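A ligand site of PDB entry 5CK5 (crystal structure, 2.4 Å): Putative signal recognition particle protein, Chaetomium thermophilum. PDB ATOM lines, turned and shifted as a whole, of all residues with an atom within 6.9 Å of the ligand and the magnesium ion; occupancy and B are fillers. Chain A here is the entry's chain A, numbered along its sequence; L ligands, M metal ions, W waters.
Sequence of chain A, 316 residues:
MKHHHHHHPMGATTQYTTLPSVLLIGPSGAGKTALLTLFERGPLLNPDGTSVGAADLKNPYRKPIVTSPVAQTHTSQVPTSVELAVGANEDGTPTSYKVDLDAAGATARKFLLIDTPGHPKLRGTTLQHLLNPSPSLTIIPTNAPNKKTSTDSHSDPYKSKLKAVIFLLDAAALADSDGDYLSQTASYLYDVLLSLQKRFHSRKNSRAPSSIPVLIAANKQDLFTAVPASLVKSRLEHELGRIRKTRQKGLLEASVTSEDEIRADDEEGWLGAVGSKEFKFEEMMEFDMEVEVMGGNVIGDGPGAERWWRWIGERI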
ATOM      1  N   GLY A  26      17.669  -2.314 -10.449  1.00  0.00           N
ATOM      2  CA  GLY A  26      16.434  -1.575 -10.392  1.00  0.00           C
ATOM      3  C   GLY A  26      15.487  -2.290  -9.456  1.00  0.00           C
ATOM      4  O   GLY A  26      15.749  -3.412  -9.077  1.00  0.00           O
ATOM      5  N   PRO A  27      14.358  -1.653  -9.135  1.00  0.00           N
ATOM      6  CA  PRO A  27      13.355  -2.150  -8.180  1.00  0.00           C
ATOM      7  C   PRO A  27      12.611  -3.382  -8.669  1.00  0.00           C
ATOM      8  O   PRO A  27      12.728  -3.726  -9.842  1.00  0.00           O
ATOM      9  CB  PRO A  27      12.391  -0.964  -8.054  1.00  0.00           C
ATOM     10  CG  PRO A  27      12.517  -0.260  -9.380  1.00  0.00           C
ATOM     11  CD  PRO A  27      13.967  -0.369  -9.735  1.00  0.00           C
ATOM     12  N   SER A  28      11.875  -4.054  -7.790  1.00  0.00           N
ATOM     13  CA  SER A  28      11.034  -5.158  -8.234  1.00  0.00           C
ATOM     14  C   SER A  28      10.073  -4.626  -9.292  1.00  0.00           C
ATOM     15  O   SER A  28       9.623  -3.489  -9.206  1.00  0.00           O
ATOM     16  CB  SER A  28      10.269  -5.763  -7.059  1.00  0.00           C
ATOM     17  OG  SER A  28      11.133  -6.330  -6.092  1.00  0.00           O
ATOM     18  N   GLY A  29       9.806  -5.413 -10.337  1.00  0.00           N
ATOM     19  CA  GLY A  29       8.767  -5.047 -11.267  1.00  0.00           C
ATOM     20  C   GLY A  29       9.120  -4.059 -12.361  1.00  0.00           C
ATOM     21  O   GLY A  29       8.227  -3.480 -12.989  1.00  0.00           O
ATOM     22  N   ALA A  30      10.403  -3.812 -12.554  1.00  0.00           N
ATOM     23  CA  ALA A  30      10.876  -2.884 -13.569  1.00  0.00           C
ATOM     24  C   ALA A  30      10.923  -3.556 -14.925  1.00  0.00           C
ATOM     25  O   ALA A  30      10.740  -2.934 -15.947  1.00  0.00           O
ATOM     26  CB  ALA A  30      12.220  -2.364 -13.209  1.00  0.00           C
ATOM     27  N   GLY A  31      11.209  -4.856 -14.893  1.00  0.00           N
ATOM     28  CA  GLY A  31      11.348  -5.635 -16.099  1.00  0.00           C
ATOM     29  C   GLY A  31      12.778  -6.084 -16.219  1.00  0.00           C
ATOM     30  O   GLY A  31      13.293  -6.182 -17.335  1.00  0.00           O
ATOM     31  N   LYS A  32      13.453  -6.300 -15.100  1.00  0.00           N
ATOM     32  CA  LYS A  32      14.878  -6.618 -15.148  1.00  0.00           C
ATOM     33  C   LYS A  32      15.011  -7.960 -15.777  1.00  0.00           C
ATOM     34  O   LYS A  32      15.663  -8.119 -16.799  1.00  0.00           O
ATOM     35  CB  LYS A  32      15.526  -6.630 -13.755  1.00  0.00           C
ATOM     36  CG  LYS A  32      15.282  -5.398 -12.930  1.00  0.00           C
ATOM     37  CD  LYS A  32      16.313  -5.243 -11.865  1.00  0.00           C
ATOM     38  CE  LYS A  32      16.203  -6.299 -10.818  1.00  0.00           C
ATOM     39  NZ  LYS A  32      14.835  -6.531 -10.314  1.00  0.00           N
ATOM     40  N   THR A  33      14.340  -8.915 -15.144  1.00  0.00           N
ATOM     41  CA  THR A  33      14.299 -10.300 -15.539  1.00  0.00           C
ATOM     42  C   THR A  33      13.746 -10.472 -16.967  1.00  0.00           C
ATOM     43  O   THR A  33      14.222 -11.294 -17.715  1.00  0.00           O
ATOM     44  CB  THR A  33      13.434 -11.098 -14.536  1.00  0.00           C
ATOM     45  OG1 THR A  33      13.723 -10.687 -13.187  1.00  0.00           O
ATOM     46  CG2 THR A  33      13.657 -12.601 -14.703  1.00  0.00           C
ATOM     47  N   ALA A  34      12.760  -9.678 -17.344  1.00  0.00           N
ATOM     48  CA  ALA A  34      12.285  -9.640 -18.727  1.00  0.00           C
ATOM     49  C   ALA A  34      13.362  -9.234 -19.751  1.00  0.00           C
ATOM     50  O   ALA A  34      13.565  -9.921 -20.750  1.00  0.00           O
ATOM     51  CB  ALA A  34      11.092  -8.709 -18.828  1.00  0.00           C
ATOM     52  N   LEU A  35      14.059  -8.124 -19.484  1.00  0.00           N
ATOM     53  CA  LEU A  35      15.069  -7.557 -20.374  1.00  0.00           C
ATOM     54  C   LEU A  35      16.233  -8.495 -20.632  1.00  0.00           C
ATOM     55  O   LEU A  35      16.842  -8.475 -21.694  1.00  0.00           O
ATOM     56  CB  LEU A  35      15.630  -6.246 -19.805  1.00  0.00           C
ATOM     57  CG  LEU A  35      16.695  -5.498 -20.612  1.00  0.00           C
ATOM     58  CD1 LEU A  35      16.139  -4.951 -21.930  1.00  0.00           C
ATOM     59  CD2 LEU A  35      17.343  -4.385 -19.838  1.00  0.00           C
ATOM     60  N   ASP A 115      21.742  -9.624 -14.110  1.00  0.00           N
ATOM     61  CA  ASP A 115      20.500  -9.415 -13.392  1.00  0.00           C
ATOM     62  C   ASP A 115      20.649  -9.414 -11.869  1.00  0.00           C
ATOM     63  O   ASP A 115      21.488 -10.113 -11.326  1.00  0.00           O
ATOM     64  CB  ASP A 115      19.504 -10.498 -13.813  1.00  0.00           C
ATOM     65  CG  ASP A 115      18.083 -10.147 -13.472  1.00  0.00           C
ATOM     66  OD1 ASP A 115      17.843  -9.123 -12.814  1.00  0.00           O
ATOM     67  OD2 ASP A 115      17.192 -10.925 -13.856  1.00  0.00           O
ATOM     68  N   THR A 116      19.811  -8.622 -11.211  1.00  0.00           N
ATOM     69  CA  THR A 116      19.838  -8.537  -9.769  1.00  0.00           C
ATOM     70  C   THR A 116      18.438  -8.823  -9.189  1.00  0.00           C
ATOM     71  O   THR A 116      17.463  -8.936  -9.938  1.00  0.00           O
ATOM     72  CB  THR A 116      20.362  -7.144  -9.344  1.00  0.00           C
ATOM     73  OG1 THR A 116      19.442  -6.127  -9.732  1.00  0.00           O
ATOM     74  CG2 THR A 116      21.716  -6.860  -9.996  1.00  0.00           C
ATOM     75  N   PRO A 117      18.331  -9.008  -7.865  1.00  0.00           N
ATOM     76  CA  PRO A 117      17.028  -9.058  -7.197  1.00  0.00           C
ATOM     77  C   PRO A 117      16.453  -7.675  -6.973  1.00  0.00           C
ATOM     78  O   PRO A 117      17.225  -6.719  -6.819  1.00  0.00           O
ATOM     79  CB  PRO A 117      17.355  -9.715  -5.843  1.00  0.00           C
ATOM     80  CG  PRO A 117      18.642 -10.392  -6.036  1.00  0.00           C
ATOM     81  CD  PRO A 117      19.395  -9.537  -7.000  1.00  0.00           C
ATOM     82  N   GLY A 118      15.137  -7.538  -6.963  1.00  0.00           N
ATOM     83  CA  GLY A 118      14.543  -6.220  -6.830  1.00  0.00           C
ATOM     84  C   GLY A 118      14.385  -5.706  -5.411  1.00  0.00           C
ATOM     85  O   GLY A 118      14.441  -4.496  -5.179  1.00  0.00           O
ATOM     86  N   LEU A 168      17.169   0.237 -14.610  1.00  0.00           N
ATOM     87  CA  LEU A 168      15.867  -0.023 -15.191  1.00  0.00           C
ATOM     88  C   LEU A 168      14.730   0.316 -14.251  1.00  0.00           C
ATOM     89  O   LEU A 168      14.747  -0.057 -13.098  1.00  0.00           O
ATOM     90  CB  LEU A 168      15.790  -1.513 -15.561  1.00  0.00           C
ATOM     91  CG  LEU A 168      14.718  -2.054 -16.494  1.00  0.00           C
ATOM     92  CD1 LEU A 168      14.745  -1.384 -17.866  1.00  0.00           C
ATOM     93  CD2 LEU A 168      14.975  -3.516 -16.647  1.00  0.00           C
ATOM     94  N   ASP A 170      10.154   1.010 -14.095  1.00  0.00           N
ATOM     95  CA  ASP A 170       8.885   0.971 -14.768  1.00  0.00           C
ATOM     96  C   ASP A 170       8.365   2.394 -14.901  1.00  0.00           C
ATOM     97  O   ASP A 170       8.039   3.041 -13.911  1.00  0.00           O
ATOM     98  CB  ASP A 170       7.931   0.086 -13.988  1.00  0.00           C
ATOM     99  CG  ASP A 170       6.667  -0.170 -14.731  1.00  0.00           C
ATOM    100  OD1 ASP A 170       6.364   0.604 -15.641  1.00  0.00           O
ATOM    101  OD2 ASP A 170       5.984  -1.162 -14.404  1.00  0.00           O
ATOM    102  N   ASN A 219      11.569   1.929 -18.829  1.00  0.00           N
ATOM    103  CA  ASN A 219      10.945   0.802 -19.512  1.00  0.00           C
ATOM    104  C   ASN A 219       9.445   0.970 -19.627  1.00  0.00           C
ATOM    105  O   ASN A 219       8.878   1.903 -19.066  1.00  0.00           O
ATOM    106  CB  ASN A 219      11.252  -0.520 -18.790  1.00  0.00           C
ATOM    107  CG  ASN A 219      11.008  -1.735 -19.673  1.00  0.00           C
ATOM    108  OD1 ASN A 219      10.902  -1.606 -20.874  1.00  0.00           O
ATOM    109  ND2 ASN A 219      10.878  -2.901 -19.075  1.00  0.00           N
ATOM    110  N   LYS A 220       8.851   0.072 -20.419  1.00  0.00           N
ATOM    111  CA  LYS A 220       7.409  -0.056 -20.622  1.00  0.00           C
ATOM    112  C   LYS A 220       6.832   1.130 -21.353  1.00  0.00           C
ATOM    113  O   LYS A 220       5.762   1.607 -20.990  1.00  0.00           O
ATOM    114  CB  LYS A 220       6.691  -0.295 -19.287  1.00  0.00           C
ATOM    115  CG  LYS A 220       7.381  -1.342 -18.421  1.00  0.00           C
ATOM    116  CD  LYS A 220       6.481  -1.988 -17.406  1.00  0.00           C
ATOM    117  CE  LYS A 220       7.244  -3.044 -16.646  1.00  0.00           C
ATOM    118  NZ  LYS A 220       6.478  -3.673 -15.538  1.00  0.00           N
ATOM    119  N   GLN A 221       7.546   1.618 -22.357  1.00  0.00           N
ATOM    120  CA  GLN A 221       7.098   2.778 -23.145  1.00  0.00           C
ATOM    121  C   GLN A 221       5.971   2.406 -24.123  1.00  0.00           C
ATOM    122  O   GLN A 221       5.433   3.276 -24.793  1.00  0.00           O
ATOM    123  CB  GLN A 221       8.273   3.364 -23.930  1.00  0.00           C
ATOM    124  CG  GLN A 221       9.337   4.056 -23.075  1.00  0.00           C
ATOM    125  CD  GLN A 221       8.832   5.291 -22.340  1.00  0.00           C
ATOM    126  OE1 GLN A 221       8.064   6.092 -22.880  1.00  0.00           O
ATOM    127  NE2 GLN A 221       9.282   5.468 -21.120  1.00  0.00           N
ATOM    128  N   ASP A 222       5.624   1.136 -24.201  1.00  0.00           N
ATOM    129  CA  ASP A 222       4.517   0.676 -25.021  1.00  0.00           C
ATOM    130  C   ASP A 222       3.146   0.938 -24.402  1.00  0.00           C
ATOM    131  O   ASP A 222       2.140   0.963 -25.094  1.00  0.00           O
ATOM    132  CB  ASP A 222       4.666  -0.818 -25.338  1.00  0.00           C
ATOM    133  CG  ASP A 222       4.753  -1.676 -24.104  1.00  0.00           C
ATOM    134  OD1 ASP A 222       5.819  -1.689 -23.449  1.00  0.00           O
ATOM    135  OD2 ASP A 222       3.745  -2.333 -23.788  1.00  0.00           O
ATOM    136  N   LEU A 223       3.099   1.109 -23.087  1.00  0.00           N
ATOM    137  CA  LEU A 223       1.858   1.408 -22.410  1.00  0.00           C
ATOM    138  C   LEU A 223       1.534   2.850 -22.657  1.00  0.00           C
ATOM    139  O   LEU A 223       2.416   3.697 -22.640  1.00  0.00           O
ATOM    140  CB  LEU A 223       1.969   1.132 -20.924  1.00  0.00           C
ATOM    141  CG  LEU A 223       2.440  -0.270 -20.597  1.00  0.00           C
ATOM    142  CD1 LEU A 223       2.868  -0.323 -19.150  1.00  0.00           C
ATOM    143  CD2 LEU A 223       1.327  -1.270 -20.890  1.00  0.00           C
ATOM    144  N   GLY A 296      12.405   3.154 -23.578  1.00  0.00           N
ATOM    145  CA  GLY A 296      12.314   1.991 -24.422  1.00  0.00           C
ATOM    146  C   GLY A 296      11.372   0.946 -23.849  1.00  0.00           C
ATOM    147  O   GLY A 296      10.774   1.176 -22.806  1.00  0.00           O
ATOM    148  N   ASN A 297      11.236  -0.188 -24.504  1.00  0.00           N
ATOM    149  CA  ASN A 297      10.381  -1.237 -23.969  1.00  0.00           C
ATOM    150  C   ASN A 297      10.852  -2.591 -24.403  1.00  0.00           C
ATOM    151  O   ASN A 297      11.521  -2.733 -25.423  1.00  0.00           O
ATOM    152  CB  ASN A 297       8.935  -1.078 -24.389  1.00  0.00           C
ATOM    153  CG  ASN A 297       8.732  -1.316 -25.845  1.00  0.00           C
ATOM    154  OD1 ASN A 297       9.137  -0.514 -26.674  1.00  0.00           O
ATOM    155  ND2 ASN A 297       8.106  -2.434 -26.172  1.00  0.00           N
ATOM    156  N   VAL A 298      10.494  -3.589 -23.607  1.00  0.00           N
ATOM    157  CA  VAL A 298      10.885  -4.969 -23.846  1.00  0.00           C
ATOM    158  C   VAL A 298       9.798  -5.761 -24.561  1.00  0.00           C
ATOM    159  O   VAL A 298      10.090  -6.491 -25.506  1.00  0.00           O
ATOM    160  CB  VAL A 298      11.200  -5.640 -22.507  1.00  0.00           C
ATOM    161  CG1 VAL A 298      11.514  -7.129 -22.699  1.00  0.00           C
ATOM    162  CG2 VAL A 298      12.336  -4.915 -21.818  1.00  0.00           C
ATOM    163  N   ILE A 299       8.545  -5.593 -24.158  1.00  0.00           N
ATOM    164  CA  ILE A 299       7.450  -6.277 -24.822  1.00  0.00           C
ATOM    165  C   ILE A 299       6.477  -5.240 -25.342  1.00  0.00           C
ATOM    166  O   ILE A 299       6.437  -4.116 -24.856  1.00  0.00           O
ATOM    167  CB  ILE A 299       6.723  -7.267 -23.894  1.00  0.00           C
ATOM    168  CG1 ILE A 299       6.043  -6.569 -22.725  1.00  0.00           C
ATOM    169  CG2 ILE A 299       7.684  -8.308 -23.372  1.00  0.00           C
ATOM    170  CD1 ILE A 299       5.281  -7.537 -21.836  1.00  0.00           C
ATOM    171  N   GLY A 300       5.714  -5.592 -26.364  1.00  0.00           N
ATOM    172  CA  GLY A 300       4.711  -4.693 -26.886  1.00  0.00           C
ATOM    173  C   GLY A 300       5.251  -3.786 -27.965  1.00  0.00           C
ATOM    174  O   GLY A 300       6.374  -3.967 -28.429  1.00  0.00           O
ATOM    175  N   TRP A 308      19.203   1.196 -26.225  1.00  0.00           N
ATOM    176  CA  TRP A 308      19.876   0.972 -24.962  1.00  0.00           C
ATOM    177  C   TRP A 308      21.222   0.296 -25.164  1.00  0.00           C
ATOM    178  O   TRP A 308      22.270   0.809 -24.786  1.00  0.00           O
ATOM    179  CB  TRP A 308      19.020   0.083 -24.068  1.00  0.00           C
ATOM    180  CG  TRP A 308      17.831   0.721 -23.507  1.00  0.00           C
ATOM    181  CD1 TRP A 308      17.636   2.045 -23.291  1.00  0.00           C
ATOM    182  CD2 TRP A 308      16.652   0.062 -23.063  1.00  0.00           C
ATOM    183  NE1 TRP A 308      16.405   2.254 -22.723  1.00  0.00           N
ATOM    184  CE2 TRP A 308      15.776   1.054 -22.583  1.00  0.00           C
ATOM    185  CE3 TRP A 308      16.253  -1.274 -23.012  1.00  0.00           C
ATOM    186  CZ2 TRP A 308      14.523   0.750 -22.075  1.00  0.00           C
ATOM    187  CZ3 TRP A 308      15.013  -1.574 -22.505  1.00  0.00           C
ATOM    188  CH2 TRP A 308      14.151  -0.563 -22.047  1.00  0.00           C
HETATM  189  P1  LIG L   1      11.737  -7.565 -12.044  1.00  0.00           P
HETATM  190  O1  LIG L   1      12.686  -8.735 -12.134  1.00  0.00           O
HETATM  191  O2  LIG L   1      10.917  -7.666 -10.787  1.00  0.00           O
HETATM  192  O3  LIG L   1      12.457  -6.274 -11.999  1.00  0.00           O
HETATM  193  O4  LIG L   1      10.730  -7.405 -13.271  1.00  0.00           O
HETATM  194  P2  LIG L   1      10.033  -8.572 -14.098  1.00  0.00           P
HETATM  195  O5  LIG L   1      10.713  -8.762 -15.402  1.00  0.00           O
HETATM  196  O6  LIG L   1       9.915  -9.861 -13.321  1.00  0.00           O
HETATM  197  O7  LIG L   1       8.554  -8.033 -14.185  1.00  0.00           O
HETATM  198  C1  LIG L   1       8.138  -6.782 -14.663  1.00  0.00           C
HETATM  199  C2  LIG L   1       6.713  -7.033 -15.118  1.00  0.00           C
HETATM  200  O8  LIG L   1       6.463  -6.073 -16.122  1.00  0.00           O
HETATM  201  C3  LIG L   1       6.611  -8.419 -15.761  1.00  0.00           C
HETATM  202  O9  LIG L   1       5.343  -9.089 -15.631  1.00  0.00           O
HETATM  203  C4  LIG L   1       6.845  -8.149 -17.219  1.00  0.00           C
HETATM  204  O10 LIG L   1       6.090  -9.064 -18.013  1.00  0.00           O
HETATM  205  C5  LIG L   1       6.330  -6.730 -17.373  1.00  0.00           C
HETATM  206  N1  LIG L   1       7.172  -6.090 -18.389  1.00  0.00           N
HETATM  207  C6  LIG L   1       8.482  -6.231 -18.572  1.00  0.00           C
HETATM  208  N2  LIG L   1       8.888  -5.469 -19.610  1.00  0.00           N
HETATM  209  C7  LIG L   1       7.808  -4.836 -20.096  1.00  0.00           C
HETATM  210  C8  LIG L   1       7.486  -3.898 -21.186  1.00  0.00           C
HETATM  211  O11 LIG L   1       8.359  -3.455 -21.955  1.00  0.00           O
HETATM  212  N3  LIG L   1       6.232  -3.512 -21.329  1.00  0.00           N
HETATM  213  C9  LIG L   1       5.255  -3.939 -20.519  1.00  0.00           C
HETATM  214  N4  LIG L   1       3.992  -3.503 -20.717  1.00  0.00           N
HETATM  215  N5  LIG L   1       5.459  -4.790 -19.524  1.00  0.00           N
HETATM  216  C10 LIG L   1       6.681  -5.263 -19.273  1.00  0.00           C
HETATM  217 MG    MG M   1      13.650 -10.254 -11.260  1.00  0.00          MG
HETATM  218  O   HOH W   1      10.543 -12.423 -12.123  1.00  0.00           O
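The backbone carbonyl oxygen (O) of Pro 27 lies close to an oxygen (O3) of the ligand. Ser 28 touches the ligand. CD2 of Leu 223 touches N4 of the ligand (3.5 Å). Asn 297 touches the ligand (CB to O11, 3.5 Å). Hydrophobic or aromatic side chains within 4 Å of the ligand: Ala 34, Leu 223, Val 298 and Ile 299. 15 residues have an atom within 4 Å of the ligand: Pro 27, Ser 28, Gly 29, Ala 30, Gly 31, Lys 32, Thr 33, Ala 34, Asn 219, Lys 220, Asp 222, Leu 223, Asn 297, Val 298 and Ile 299.
The side-chain amino group (NZ) of Lys 220 lies within hydrogen-bond range of the backbone carbonyl oxygen (O) of Gly 29, at 3.1 Å. The backbone NH of Val 298 sits at hydrogen-bond distance from the side-chain amide oxygen of Asn 219, at 3.4 Å. NZ of Lys 32 sits close to O of Gly 26 (3.5 Å). N of Lys 220 is in hydrogen-bond range of O of Gly 296, at 3.3 Å. The side-chain amide nitrogen (ND2) of Asn 297 lies within hydrogen-bond range of the backbone carbonyl oxygen (O) of Gly 300, 3.2 Å away. The side-chain carboxylate (OD2) of Asp 170 lies within salt-bridge range of the side-chain amino group (NZ) of Lys 220 (2.8 Å). The backbone carbonyl oxygen (O) of Ile 299 is in hydrogen-bond range of the side-chain amide nitrogen (ND2) of Asn 297. ND2 of Asn 219 lies within hydrogen-bond range of O of Ala 30, at 3.1 Å.
The magnesium ion is bound by the side-chain hydroxyl of Thr 33 (2.0 Å) and an oxygen (O1) of the ligand (2.0 Å). The magnesium ion has two donor atoms within binding distance.
The backbone NH (N) of Lys 32 lies close to an oxygen (O3) of the ligand, 3.3 Å away. N of Thr 33 sits close to O1 of the ligand (3.4 Å). NZ of Lys 220 sits at hydrogen-bond distance from O8 of the ligand (2.5 Å). The side-chain carboxylate (OD1) of Asp 222 sits at hydrogen-bond distance from a nitrogen (N3) of the ligand (2.8 Å). O11 of the ligand sits at hydrogen-bond distance from N of Ile 299 (3.1 Å). The side-chain amide nitrogen of Asn 219 sits at hydrogen-bond distance from a nitrogen (N2) of the ligand, 3.3 Å away. O11 of the ligand is in hydrogen-bond range of N of Val 298 (2.7 Å). O4 of the ligand is in hydrogen-bond range of N of Gly 31, at 3.1 Å. An oxygen (O5) of the ligand is in hydrogen-bond range of the backbone NH of Ala 34 (3.0 Å). The side-chain amino group of Lys 32 is in salt-bridge range of an oxygen (O3) of the ligand, 2.9 Å away. The backbone NH of Ala 30 sits at hydrogen-bond distance from an oxygen (O3) of the ligand (3.3 Å). N of Gly 29 is in hydrogen-bond range of O2 of the ligand (2.6 Å).
The nearest printed residue that does not touch the magnesium ion is Lys 32 (4.02 Å).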
